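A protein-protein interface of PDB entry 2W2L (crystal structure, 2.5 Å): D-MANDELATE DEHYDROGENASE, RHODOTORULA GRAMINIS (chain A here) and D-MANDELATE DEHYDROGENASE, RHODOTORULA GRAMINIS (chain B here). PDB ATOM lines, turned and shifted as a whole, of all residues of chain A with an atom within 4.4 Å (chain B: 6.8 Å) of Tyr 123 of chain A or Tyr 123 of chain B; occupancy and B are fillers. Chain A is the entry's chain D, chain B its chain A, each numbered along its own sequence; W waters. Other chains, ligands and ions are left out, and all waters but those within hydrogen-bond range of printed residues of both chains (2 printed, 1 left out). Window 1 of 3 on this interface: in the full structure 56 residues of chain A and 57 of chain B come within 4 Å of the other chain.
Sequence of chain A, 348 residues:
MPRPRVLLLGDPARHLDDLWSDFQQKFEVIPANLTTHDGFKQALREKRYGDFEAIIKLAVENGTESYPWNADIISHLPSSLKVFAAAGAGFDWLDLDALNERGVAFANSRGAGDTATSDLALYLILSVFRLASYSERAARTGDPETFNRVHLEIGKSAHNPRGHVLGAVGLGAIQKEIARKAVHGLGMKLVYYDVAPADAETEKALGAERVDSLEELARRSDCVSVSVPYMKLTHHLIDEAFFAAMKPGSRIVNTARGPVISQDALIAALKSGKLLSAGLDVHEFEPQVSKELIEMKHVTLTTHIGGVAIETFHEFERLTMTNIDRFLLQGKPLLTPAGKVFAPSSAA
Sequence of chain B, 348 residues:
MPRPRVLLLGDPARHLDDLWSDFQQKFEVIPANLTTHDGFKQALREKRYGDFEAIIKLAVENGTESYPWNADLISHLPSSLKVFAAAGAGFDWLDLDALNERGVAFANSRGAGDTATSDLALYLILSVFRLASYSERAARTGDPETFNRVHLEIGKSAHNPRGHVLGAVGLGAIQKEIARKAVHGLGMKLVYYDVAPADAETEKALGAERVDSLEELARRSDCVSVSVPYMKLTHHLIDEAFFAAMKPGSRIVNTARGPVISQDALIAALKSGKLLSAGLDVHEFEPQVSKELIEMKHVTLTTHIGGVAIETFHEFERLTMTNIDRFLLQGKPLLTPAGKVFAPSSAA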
ATOM      1  N   ASP A 119     -25.547 -18.504 -34.337  1.00  0.00           N
ATOM      2  CA  ASP A 119     -26.242 -19.070 -33.171  1.00  0.00           C
ATOM      3  C   ASP A 119     -25.319 -19.808 -32.175  1.00  0.00           C
ATOM      4  O   ASP A 119     -25.407 -19.624 -30.969  1.00  0.00           O
ATOM      5  CB  ASP A 119     -27.289 -20.066 -33.647  1.00  0.00           C
ATOM      6  CG  ASP A 119     -28.564 -19.401 -34.114  1.00  0.00           C
ATOM      7  OD1 ASP A 119     -28.671 -18.140 -33.973  1.00  0.00           O
ATOM      8  OD2 ASP A 119     -29.442 -20.172 -34.607  1.00  0.00           O
ATOM      9  N   LEU A 120     -24.456 -20.659 -32.695  1.00  0.00           N
ATOM     10  CA  LEU A 120     -23.514 -21.404 -31.902  1.00  0.00           C
ATOM     11  C   LEU A 120     -22.619 -20.406 -31.164  1.00  0.00           C
ATOM     12  O   LEU A 120     -22.415 -20.509 -29.957  1.00  0.00           O
ATOM     13  CB  LEU A 120     -22.732 -22.315 -32.839  1.00  0.00           C
ATOM     14  CG  LEU A 120     -22.101 -23.544 -32.262  1.00  0.00           C
ATOM     15  CD1 LEU A 120     -20.654 -23.264 -31.930  1.00  0.00           C
ATOM     16  CD2 LEU A 120     -22.902 -23.987 -31.052  1.00  0.00           C
ATOM     17  N   ALA A 121     -22.166 -19.390 -31.893  1.00  0.00           N
ATOM     18  CA  ALA A 121     -21.354 -18.324 -31.332  1.00  0.00           C
ATOM     19  C   ALA A 121     -22.113 -17.592 -30.217  1.00  0.00           C
ATOM     20  O   ALA A 121     -21.528 -17.298 -29.161  1.00  0.00           O
ATOM     21  CB  ALA A 121     -20.941 -17.353 -32.436  1.00  0.00           C
ATOM     22  N   LEU A 122     -23.392 -17.269 -30.453  1.00  0.00           N
ATOM     23  CA  LEU A 122     -24.226 -16.748 -29.369  1.00  0.00           C
ATOM     24  C   LEU A 122     -24.304 -17.737 -28.185  1.00  0.00           C
ATOM     25  O   LEU A 122     -24.316 -17.318 -27.030  1.00  0.00           O
ATOM     26  CB  LEU A 122     -25.632 -16.351 -29.853  1.00  0.00           C
ATOM     27  CG  LEU A 122     -26.379 -15.340 -28.971  1.00  0.00           C
ATOM     28  CD1 LEU A 122     -25.830 -13.920 -29.086  1.00  0.00           C
ATOM     29  CD2 LEU A 122     -27.859 -15.341 -29.251  1.00  0.00           C
ATOM     30  N   TYR A 123     -24.285 -19.033 -28.464  1.00  0.00           N
ATOM     31  CA  TYR A 123     -24.306 -20.011 -27.422  1.00  0.00           C
ATOM     32  C   TYR A 123     -23.043 -19.977 -26.573  1.00  0.00           C
ATOM     33  O   TYR A 123     -23.088 -20.139 -25.344  1.00  0.00           O
ATOM     34  CB  TYR A 123     -24.409 -21.362 -28.080  1.00  0.00           C
ATOM     35  CG  TYR A 123     -24.166 -22.535 -27.208  1.00  0.00           C
ATOM     36  CD1 TYR A 123     -25.196 -23.077 -26.467  1.00  0.00           C
ATOM     37  CD2 TYR A 123     -22.924 -23.154 -27.183  1.00  0.00           C
ATOM     38  CE1 TYR A 123     -24.999 -24.202 -25.661  1.00  0.00           C
ATOM     39  CE2 TYR A 123     -22.705 -24.277 -26.384  1.00  0.00           C
ATOM     40  CZ  TYR A 123     -23.757 -24.785 -25.637  1.00  0.00           C
ATOM     41  OH  TYR A 123     -23.577 -25.886 -24.883  1.00  0.00           O
ATOM     42  N   LEU A 124     -21.920 -19.781 -27.258  1.00  0.00           N
ATOM     43  CA  LEU A 124     -20.586 -19.699 -26.650  1.00  0.00           C
ATOM     44  C   LEU A 124     -20.435 -18.504 -25.767  1.00  0.00           C
ATOM     45  O   LEU A 124     -19.823 -18.589 -24.677  1.00  0.00           O
ATOM     46  CB  LEU A 124     -19.534 -19.659 -27.745  1.00  0.00           C
ATOM     47  CG  LEU A 124     -19.466 -20.988 -28.503  1.00  0.00           C
ATOM     48  CD1 LEU A 124     -18.541 -20.887 -29.698  1.00  0.00           C
ATOM     49  CD2 LEU A 124     -19.023 -22.154 -27.580  1.00  0.00           C
ATOM     50  N   ILE A 125     -21.008 -17.391 -26.207  1.00  0.00           N
ATOM     51  CA  ILE A 125     -20.869 -16.136 -25.483  1.00  0.00           C
ATOM     52  C   ILE A 125     -21.659 -16.245 -24.208  1.00  0.00           C
ATOM     53  O   ILE A 125     -21.174 -15.859 -23.107  1.00  0.00           O
ATOM     54  CB  ILE A 125     -21.366 -14.951 -26.324  1.00  0.00           C
ATOM     55  CG1 ILE A 125     -20.441 -14.769 -27.531  1.00  0.00           C
ATOM     56  CG2 ILE A 125     -21.458 -13.668 -25.510  1.00  0.00           C
ATOM     57  CD1 ILE A 125     -20.976 -13.770 -28.527  1.00  0.00           C
ATOM     58  N   LEU A 126     -22.860 -16.802 -24.347  1.00  0.00           N
ATOM     59  CA  LEU A 126     -23.677 -17.145 -23.175  1.00  0.00           C
ATOM     60  C   LEU A 126     -22.880 -18.051 -22.265  1.00  0.00           C
ATOM     61  O   LEU A 126     -22.889 -17.900 -21.072  1.00  0.00           O
ATOM     62  CB  LEU A 126     -25.043 -17.768 -23.544  1.00  0.00           C
ATOM     63  CG  LEU A 126     -25.984 -16.737 -24.227  1.00  0.00           C
ATOM     64  CD1 LEU A 126     -27.209 -17.364 -24.915  1.00  0.00           C
ATOM     65  CD2 LEU A 126     -26.426 -15.659 -23.250  1.00  0.00           C
ATOM     66  N   SER A 127     -22.133 -18.953 -22.833  1.00  0.00           N
ATOM     67  CA  SER A 127     -21.592 -19.983 -22.020  1.00  0.00           C
ATOM     68  C   SER A 127     -20.434 -19.438 -21.194  1.00  0.00           C
ATOM     69  O   SER A 127     -20.350 -19.729 -20.009  1.00  0.00           O
ATOM     70  CB  SER A 127     -21.167 -21.175 -22.869  1.00  0.00           C
ATOM     71  OG  SER A 127     -20.430 -22.031 -22.060  1.00  0.00           O
ATOM     72  N   ALA A 132     -21.606 -21.752 -17.985  1.00  0.00           N
ATOM     73  CA  ALA A 132     -22.661 -22.739 -18.092  1.00  0.00           C
ATOM     74  C   ALA A 132     -22.065 -24.098 -18.332  1.00  0.00           C
ATOM     75  O   ALA A 132     -22.610 -25.093 -17.890  1.00  0.00           O
ATOM     76  CB  ALA A 132     -23.620 -22.385 -19.162  1.00  0.00           C
ATOM     77  N   SER A 133     -20.912 -24.125 -18.982  1.00  0.00           N
ATOM     78  CA  SER A 133     -20.174 -25.354 -19.208  1.00  0.00           C
ATOM     79  C   SER A 133     -19.827 -26.129 -17.940  1.00  0.00           C
ATOM     80  O   SER A 133     -20.085 -27.320 -17.835  1.00  0.00           O
ATOM     81  CB  SER A 133     -18.891 -25.009 -19.909  1.00  0.00           C
ATOM     82  OG  SER A 133     -18.312 -26.200 -20.382  1.00  0.00           O
ATOM     83  N   GLU A 136     -22.908 -27.492 -16.295  1.00  0.00           N
ATOM     84  CA  GLU A 136     -23.413 -28.760 -16.866  1.00  0.00           C
ATOM     85  C   GLU A 136     -22.597 -29.955 -16.393  1.00  0.00           C
ATOM     86  O   GLU A 136     -23.163 -31.007 -16.111  1.00  0.00           O
ATOM     87  CB  GLU A 136     -23.450 -28.787 -18.406  1.00  0.00           C
ATOM     88  CG  GLU A 136     -24.305 -27.699 -19.088  1.00  0.00           C
ATOM     89  CD  GLU A 136     -24.716 -28.062 -20.540  1.00  0.00           C
ATOM     90  OE1 GLU A 136     -24.418 -29.167 -21.012  1.00  0.00           O
ATOM     91  OE2 GLU A 136     -25.358 -27.240 -21.210  1.00  0.00           O
ATOM     92  N   SER B 118     -33.804 -15.112 -18.365  1.00  0.00           N
ATOM     93  CA  SER B 118     -34.157 -15.182 -19.779  1.00  0.00           C
ATOM     94  C   SER B 118     -32.962 -15.656 -20.637  1.00  0.00           C
ATOM     95  O   SER B 118     -33.113 -16.554 -21.486  1.00  0.00           O
ATOM     96  CB  SER B 118     -34.844 -13.918 -20.285  1.00  0.00           C
ATOM     97  OG  SER B 118     -34.066 -12.782 -20.115  1.00  0.00           O
ATOM     98  N   ASP B 119     -31.769 -15.145 -20.337  1.00  0.00           N
ATOM     99  CA  ASP B 119     -30.558 -15.521 -21.076  1.00  0.00           C
ATOM    100  C   ASP B 119     -30.218 -16.995 -20.891  1.00  0.00           C
ATOM    101  O   ASP B 119     -29.737 -17.664 -21.820  1.00  0.00           O
ATOM    102  CB  ASP B 119     -29.364 -14.645 -20.674  1.00  0.00           C
ATOM    103  CG  ASP B 119     -29.375 -13.210 -21.344  1.00  0.00           C
ATOM    104  OD1 ASP B 119     -30.266 -12.825 -22.186  1.00  0.00           O
ATOM    105  OD2 ASP B 119     -28.443 -12.423 -20.991  1.00  0.00           O
ATOM    106  N   LEU B 120     -30.482 -17.516 -19.702  1.00  0.00           N
ATOM    107  CA  LEU B 120     -30.141 -18.898 -19.447  1.00  0.00           C
ATOM    108  C   LEU B 120     -31.138 -19.786 -20.205  1.00  0.00           C
ATOM    109  O   LEU B 120     -30.798 -20.881 -20.609  1.00  0.00           O
ATOM    110  CB  LEU B 120     -30.097 -19.197 -17.943  1.00  0.00           C
ATOM    111  CG  LEU B 120     -29.466 -20.507 -17.406  1.00  0.00           C
ATOM    112  CD1 LEU B 120     -30.462 -21.656 -17.370  1.00  0.00           C
ATOM    113  CD2 LEU B 120     -28.176 -20.921 -18.134  1.00  0.00           C
ATOM    114  N   ALA B 121     -32.339 -19.290 -20.472  1.00  0.00           N
ATOM    115  CA  ALA B 121     -33.302 -20.131 -21.154  1.00  0.00           C
ATOM    116  C   ALA B 121     -33.006 -20.164 -22.637  1.00  0.00           C
ATOM    117  O   ALA B 121     -33.068 -21.231 -23.296  1.00  0.00           O
ATOM    118  CB  ALA B 121     -34.676 -19.653 -20.910  1.00  0.00           C
ATOM    119  N   LEU B 122     -32.679 -18.999 -23.162  1.00  0.00           N
ATOM    120  CA  LEU B 122     -32.259 -18.878 -24.520  1.00  0.00           C
ATOM    121  C   LEU B 122     -31.083 -19.851 -24.760  1.00  0.00           C
ATOM    122  O   LEU B 122     -31.124 -20.631 -25.721  1.00  0.00           O
ATOM    123  CB  LEU B 122     -31.890 -17.431 -24.813  1.00  0.00           C
ATOM    124  CG  LEU B 122     -31.638 -17.256 -26.301  1.00  0.00           C
ATOM    125  CD1 LEU B 122     -32.983 -16.985 -27.092  1.00  0.00           C
ATOM    126  CD2 LEU B 122     -30.677 -16.117 -26.433  1.00  0.00           C
ATOM    127  N   TYR B 123     -30.085 -19.841 -23.870  1.00  0.00           N
ATOM    128  CA  TYR B 123     -28.963 -20.801 -23.889  1.00  0.00           C
ATOM    129  C   TYR B 123     -29.479 -22.195 -23.997  1.00  0.00           C
ATOM    130  O   TYR B 123     -28.957 -22.983 -24.790  1.00  0.00           O
ATOM    131  CB  TYR B 123     -28.118 -20.749 -22.597  1.00  0.00           C
ATOM    132  CG  TYR B 123     -27.069 -21.882 -22.371  1.00  0.00           C
ATOM    133  CD1 TYR B 123     -25.751 -21.744 -22.796  1.00  0.00           C
ATOM    134  CD2 TYR B 123     -27.393 -23.047 -21.694  1.00  0.00           C
ATOM    135  CE1 TYR B 123     -24.817 -22.728 -22.586  1.00  0.00           C
ATOM    136  CE2 TYR B 123     -26.441 -24.062 -21.459  1.00  0.00           C
ATOM    137  CZ  TYR B 123     -25.174 -23.880 -21.894  1.00  0.00           C
ATOM    138  OH  TYR B 123     -24.236 -24.843 -21.662  1.00  0.00           O
ATOM    139  N   LEU B 124     -30.477 -22.534 -23.183  1.00  0.00           N
ATOM    140  CA  LEU B 124     -30.955 -23.918 -23.180  1.00  0.00           C
ATOM    141  C   LEU B 124     -31.699 -24.213 -24.462  1.00  0.00           C
ATOM    142  O   LEU B 124     -31.674 -25.337 -24.941  1.00  0.00           O
ATOM    143  CB  LEU B 124     -31.875 -24.190 -21.999  1.00  0.00           C
ATOM    144  CG  LEU B 124     -31.364 -24.064 -20.578  1.00  0.00           C
ATOM    145  CD1 LEU B 124     -32.555 -23.883 -19.678  1.00  0.00           C
ATOM    146  CD2 LEU B 124     -30.562 -25.314 -20.192  1.00  0.00           C
ATOM    147  N   ILE B 125     -32.399 -23.210 -24.984  1.00  0.00           N
ATOM    148  CA  ILE B 125     -33.115 -23.376 -26.230  1.00  0.00           C
ATOM    149  C   ILE B 125     -32.103 -23.667 -27.346  1.00  0.00           C
ATOM    150  O   ILE B 125     -32.250 -24.646 -28.099  1.00  0.00           O
ATOM    151  CB  ILE B 125     -33.924 -22.141 -26.554  1.00  0.00           C
ATOM    152  CG1 ILE B 125     -35.103 -22.016 -25.589  1.00  0.00           C
ATOM    153  CG2 ILE B 125     -34.379 -22.177 -28.006  1.00  0.00           C
ATOM    154  CD1 ILE B 125     -35.790 -20.622 -25.625  1.00  0.00           C
ATOM    155  N   LEU B 126     -31.055 -22.849 -27.427  1.00  0.00           N
ATOM    156  CA  LEU B 126     -29.947 -23.113 -28.347  1.00  0.00           C
ATOM    157  C   LEU B 126     -29.462 -24.521 -28.120  1.00  0.00           C
ATOM    158  O   LEU B 126     -29.297 -25.286 -29.063  1.00  0.00           O
ATOM    159  CB  LEU B 126     -28.813 -22.089 -28.204  1.00  0.00           C
ATOM    160  CG  LEU B 126     -29.197 -20.680 -28.716  1.00  0.00           C
ATOM    161  CD1 LEU B 126     -28.341 -19.574 -28.135  1.00  0.00           C
ATOM    162  CD2 LEU B 126     -29.135 -20.610 -30.239  1.00  0.00           C
ATOM    163  N   SER B 127     -29.329 -24.915 -26.872  1.00  0.00           N
ATOM    164  CA  SER B 127     -28.784 -26.245 -26.587  1.00  0.00           C
ATOM    165  C   SER B 127     -29.653 -27.408 -27.098  1.00  0.00           C
ATOM    166  O   SER B 127     -29.115 -28.409 -27.562  1.00  0.00           O
ATOM    167  CB  SER B 127     -28.488 -26.406 -25.109  1.00  0.00           C
ATOM    168  OG  SER B 127     -27.844 -27.642 -24.940  1.00  0.00           O
ATOM    169  N   VAL B 128     -30.976 -27.251 -27.059  1.00  0.00           N
ATOM    170  CA  VAL B 128     -31.853 -28.332 -27.499  1.00  0.00           C
ATOM    171  C   VAL B 128     -32.225 -28.296 -28.989  1.00  0.00           C
ATOM    172  O   VAL B 128     -32.678 -29.305 -29.546  1.00  0.00           O
ATOM    173  CB  VAL B 128     -33.120 -28.535 -26.581  1.00  0.00           C
ATOM    174  CG1 VAL B 128     -32.710 -28.764 -25.127  1.00  0.00           C
ATOM    175  CG2 VAL B 128     -34.137 -27.385 -26.720  1.00  0.00           C
ATOM    176  N   ARG B 130     -29.661 -27.587 -31.117  1.00  0.00           N
ATOM    177  CA  ARG B 130     -28.374 -27.850 -31.725  1.00  0.00           C
ATOM    178  C   ARG B 130     -27.672 -29.023 -31.120  1.00  0.00           C
ATOM    179  O   ARG B 130     -26.586 -29.382 -31.555  1.00  0.00           O
ATOM    180  CB  ARG B 130     -27.471 -26.608 -31.615  1.00  0.00           C
ATOM    181  CG  ARG B 130     -28.158 -25.310 -32.052  1.00  0.00           C
ATOM    182  CD  ARG B 130     -28.369 -25.259 -33.589  1.00  0.00           C
ATOM    183  NE  ARG B 130     -27.066 -25.458 -34.191  1.00  0.00           N
ATOM    184  CZ  ARG B 130     -26.342 -24.501 -34.745  1.00  0.00           C
ATOM    185  NH1 ARG B 130     -26.788 -23.263 -34.802  1.00  0.00           N
ATOM    186  NH2 ARG B 130     -25.154 -24.790 -35.201  1.00  0.00           N
ATOM    187  N   LEU B 131     -28.270 -29.621 -30.106  1.00  0.00           N
ATOM    188  CA  LEU B 131     -27.619 -30.744 -29.379  1.00  0.00           C
ATOM    189  C   LEU B 131     -26.176 -30.387 -28.929  1.00  0.00           C
ATOM    190  O   LEU B 131     -25.226 -31.175 -29.115  1.00  0.00           O
ATOM    191  CB  LEU B 131     -27.651 -32.056 -30.223  1.00  0.00           C
ATOM    192  CG  LEU B 131     -29.061 -32.451 -30.654  1.00  0.00           C
ATOM    193  CD1 LEU B 131     -29.073 -33.499 -31.742  1.00  0.00           C
ATOM    194  CD2 LEU B 131     -29.953 -32.916 -29.477  1.00  0.00           C
ATOM    195  N   ALA B 132     -26.014 -29.207 -28.340  1.00  0.00           N
ATOM    196  CA  ALA B 132     -24.669 -28.734 -28.001  1.00  0.00           C
ATOM    197  C   ALA B 132     -24.099 -29.469 -26.793  1.00  0.00           C
ATOM    198  O   ALA B 132     -22.886 -29.694 -26.690  1.00  0.00           O
ATOM    199  CB  ALA B 132     -24.710 -27.271 -27.738  1.00  0.00           C
ATOM    200  N   SER B 133     -24.994 -29.843 -25.879  1.00  0.00           N
ATOM    201  CA  SER B 133     -24.599 -30.593 -24.668  1.00  0.00           C
ATOM    202  C   SER B 133     -23.928 -31.888 -25.023  1.00  0.00           C
ATOM    203  O   SER B 133     -22.884 -32.196 -24.524  1.00  0.00           O
ATOM    204  CB  SER B 133     -25.827 -30.925 -23.842  1.00  0.00           C
ATOM    205  OG  SER B 133     -25.518 -30.799 -22.493  1.00  0.00           O
ATOM    206  N   GLU B 136     -20.579 -30.975 -26.504  1.00  0.00           N
ATOM    207  CA  GLU B 136     -19.612 -30.733 -25.441  1.00  0.00           C
ATOM    208  C   GLU B 136     -18.977 -31.982 -24.847  1.00  0.00           C
ATOM    209  O   GLU B 136     -17.756 -32.065 -24.745  1.00  0.00           O
ATOM    210  CB  GLU B 136     -20.234 -29.930 -24.326  1.00  0.00           C
ATOM    211  CG  GLU B 136     -20.508 -28.541 -24.760  1.00  0.00           C
ATOM    212  CD  GLU B 136     -20.343 -27.557 -23.636  1.00  0.00           C
ATOM    213  OE1 GLU B 136     -19.414 -27.768 -22.795  1.00  0.00           O
ATOM    214  OE2 GLU B 136     -21.136 -26.566 -23.624  1.00  0.00           O
ATOM    215  N   VAL B 253     -37.802 -26.920 -22.567  1.00  0.00           N
ATOM    216  CA  VAL B 253     -36.892 -26.335 -21.548  1.00  0.00           C
ATOM    217  C   VAL B 253     -37.624 -25.794 -20.318  1.00  0.00           C
ATOM    218  O   VAL B 253     -38.684 -25.112 -20.405  1.00  0.00           O
ATOM    219  CB  VAL B 253     -35.946 -25.214 -22.124  1.00  0.00           C
ATOM    220  CG1 VAL B 253     -35.145 -25.759 -23.293  1.00  0.00           C
ATOM    221  CG2 VAL B 253     -36.757 -23.966 -22.547  1.00  0.00           C
ATOM    222  N   THR B 300     -29.955 -31.546 -21.742  1.00  0.00           N
ATOM    223  CA  THR B 300     -29.041 -30.549 -21.198  1.00  0.00           C
ATOM    224  C   THR B 300     -29.399 -30.334 -19.745  1.00  0.00           C
ATOM    225  O   THR B 300     -30.575 -30.142 -19.411  1.00  0.00           O
ATOM    226  CB  THR B 300     -29.113 -29.231 -22.032  1.00  0.00           C
ATOM    227  OG1 THR B 300     -28.755 -29.530 -23.381  1.00  0.00           O
ATOM    228  CG2 THR B 300     -28.157 -28.197 -21.540  1.00  0.00           C
ATOM    229  N   THR B 302     -28.390 -28.127 -16.068  1.00  0.00           N
ATOM    230  CA  THR B 302     -27.576 -27.212 -15.278  1.00  0.00           C
ATOM    231  C   THR B 302     -28.005 -27.084 -13.818  1.00  0.00           C
ATOM    232  O   THR B 302     -29.179 -27.333 -13.506  1.00  0.00           O
ATOM    233  CB  THR B 302     -27.566 -25.791 -15.831  1.00  0.00           C
ATOM    234  OG1 THR B 302     -28.907 -25.345 -15.898  1.00  0.00           O
ATOM    235  CG2 THR B 302     -26.882 -25.719 -17.193  1.00  0.00           C
ATOM    236  N   ILE B 305     -28.786 -22.388 -12.389  1.00  0.00           N
ATOM    237  CA  ILE B 305     -28.061 -21.128 -12.537  1.00  0.00           C
ATOM    238  C   ILE B 305     -28.853 -20.035 -13.272  1.00  0.00           C
ATOM    239  O   ILE B 305     -28.265 -19.052 -13.703  1.00  0.00           O
ATOM    240  CB  ILE B 305     -26.643 -21.314 -13.167  1.00  0.00           C
ATOM    241  CG1 ILE B 305     -26.763 -21.730 -14.652  1.00  0.00           C
ATOM    242  CG2 ILE B 305     -25.736 -22.302 -12.276  1.00  0.00           C
ATOM    243  CD1 ILE B 305     -25.439 -22.094 -15.358  1.00  0.00           C
HETATM  244  O   HOH W   1     -25.464 -27.331 -23.871  1.00  0.00           O
HETATM  245  O   HOH W   2     -21.661 -24.646 -22.015  1.00  0.00           O
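OE2 of Glu 136 of chain A lies within hydrogen-bond range of OH of Tyr 123 of chain B (2.7 Å).
The side-chain hydroxyl of Ser 133 of chain A lies within hydrogen-bond range of the side-chain carboxylate of Glu 136 of chain B.
The side-chain hydroxyl of Tyr 123 of chain A sits at hydrogen-bond distance from the side-chain hydroxyl of Tyr 123 of chain B (3.4 Å).
OG of Ser 133 of chain B lies within hydrogen-bond range of OE1 of Glu 136 of chain A, 2.5 Å away.
OE2 of Glu 136 of chain B sits at hydrogen-bond distance from OH of Tyr 123 of chain A (2.8 Å).
OG of Ser 127 of chain B lies within hydrogen-bond range of OG1 of Thr 300 of chain B (2.6 Å).
The backbone NH (N) of Ala 132 of chain A sits at hydrogen-bond distance from the backbone carbonyl oxygen (O) of Ser 127 of chain A (3.1 Å).
The backbone carbonyl oxygen (O) of Ser 127 of chain B is in hydrogen-bond range of the backbone NH (N) of Ala 132 of chain B (3.3 Å).
Among the printed residues, merely in contact across the chains: Glu 136 of chain A with Thr 300 of chain B (3.0 Å), Tyr 123 of chain A with Ala 132 of chain B (3.4 Å), Asp 119 of chain A with Arg 130 of chain B (3.4 Å), Ala 132 of chain A with Tyr 123 of chain B (3.5 Å), Glu 136 of chain A with Thr 302 of chain B (3.8 Å), Asp 119 of chain A with Leu 126 of chain B (3.9 Å), Leu 126 of chain A with Tyr 123 of chain B (3.9 Å), Ala 132 of chain A with Ile 305 of chain B (3.95 Å), Ser 127 of chain A with Tyr 123 of chain B (3.98 Å) and Leu 126 of chain A with Leu 122 of chain B (3.99 Å).
Of the printed residues of chain B, Asp 119 of chain A touches Leu 126 (3.9 Å) and Arg 130 (3.4 Å).
Of chain B, only Tyr 123, Ala 132 and Glu 136 come within 4 Å of Tyr 123 of chain A.
Of the printed residues of chain B, Ser 133 of chain A touches Glu 136 (3.1 Å).
Ala 121 of chain B touches none of the printed residues of chain A.
Printed residues of chain A within 4 Å of Leu 122 of chain B: Leu 126 (3.99 Å).
Tyr 123 of chain B touches just these residues of chain A: Tyr 123 (3.4 Å), Leu 126 (3.9 Å), Ser 127 (3.98 Å), Ala 132 (3.5 Å) and Glu 136 (2.7 Å).
Ser 127 of chain B touches none of the printed residues of chain A.
Printed residues of chain A within 4 Å of Ala 132 of chain B: Tyr 123.
Printed residues of chain A within 4 Å of Ile 305 of chain B: Ala 132.
The nearest residue of chain B that does not touch Tyr 123 of chain A is Leu 126 of chain B (4.1 Å).
The nearest residue of chain A that does not touch Tyr 123 of chain B is Ser 133 of chain A (4.3 Å).
Hydrophobic or aromatic side chains of chain A that line the printed part of chain B: Tyr 123, Leu 126 and Ala 132.
Water W2 lies within hydrogen-bond range of OE2 of Glu 136 of chain B (2.6 Å), OH of Tyr 123 of chain B (2.6 Å), OG of Ser 127 of chain A (2.9 Å) and N of Ser 133 of chain A (3.2 Å).
Water W1 lies within hydrogen-bond range of the side-chain hydroxyl of Tyr 123 of chain A (2.6 Å), the side-chain hydroxyl of Ser 127 of chain B (2.6 Å), the side-chain carboxylate of Glu 136 of chain A (2.7 Å) and the backbone NH of Ser 133 of chain B (3.3 Å).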
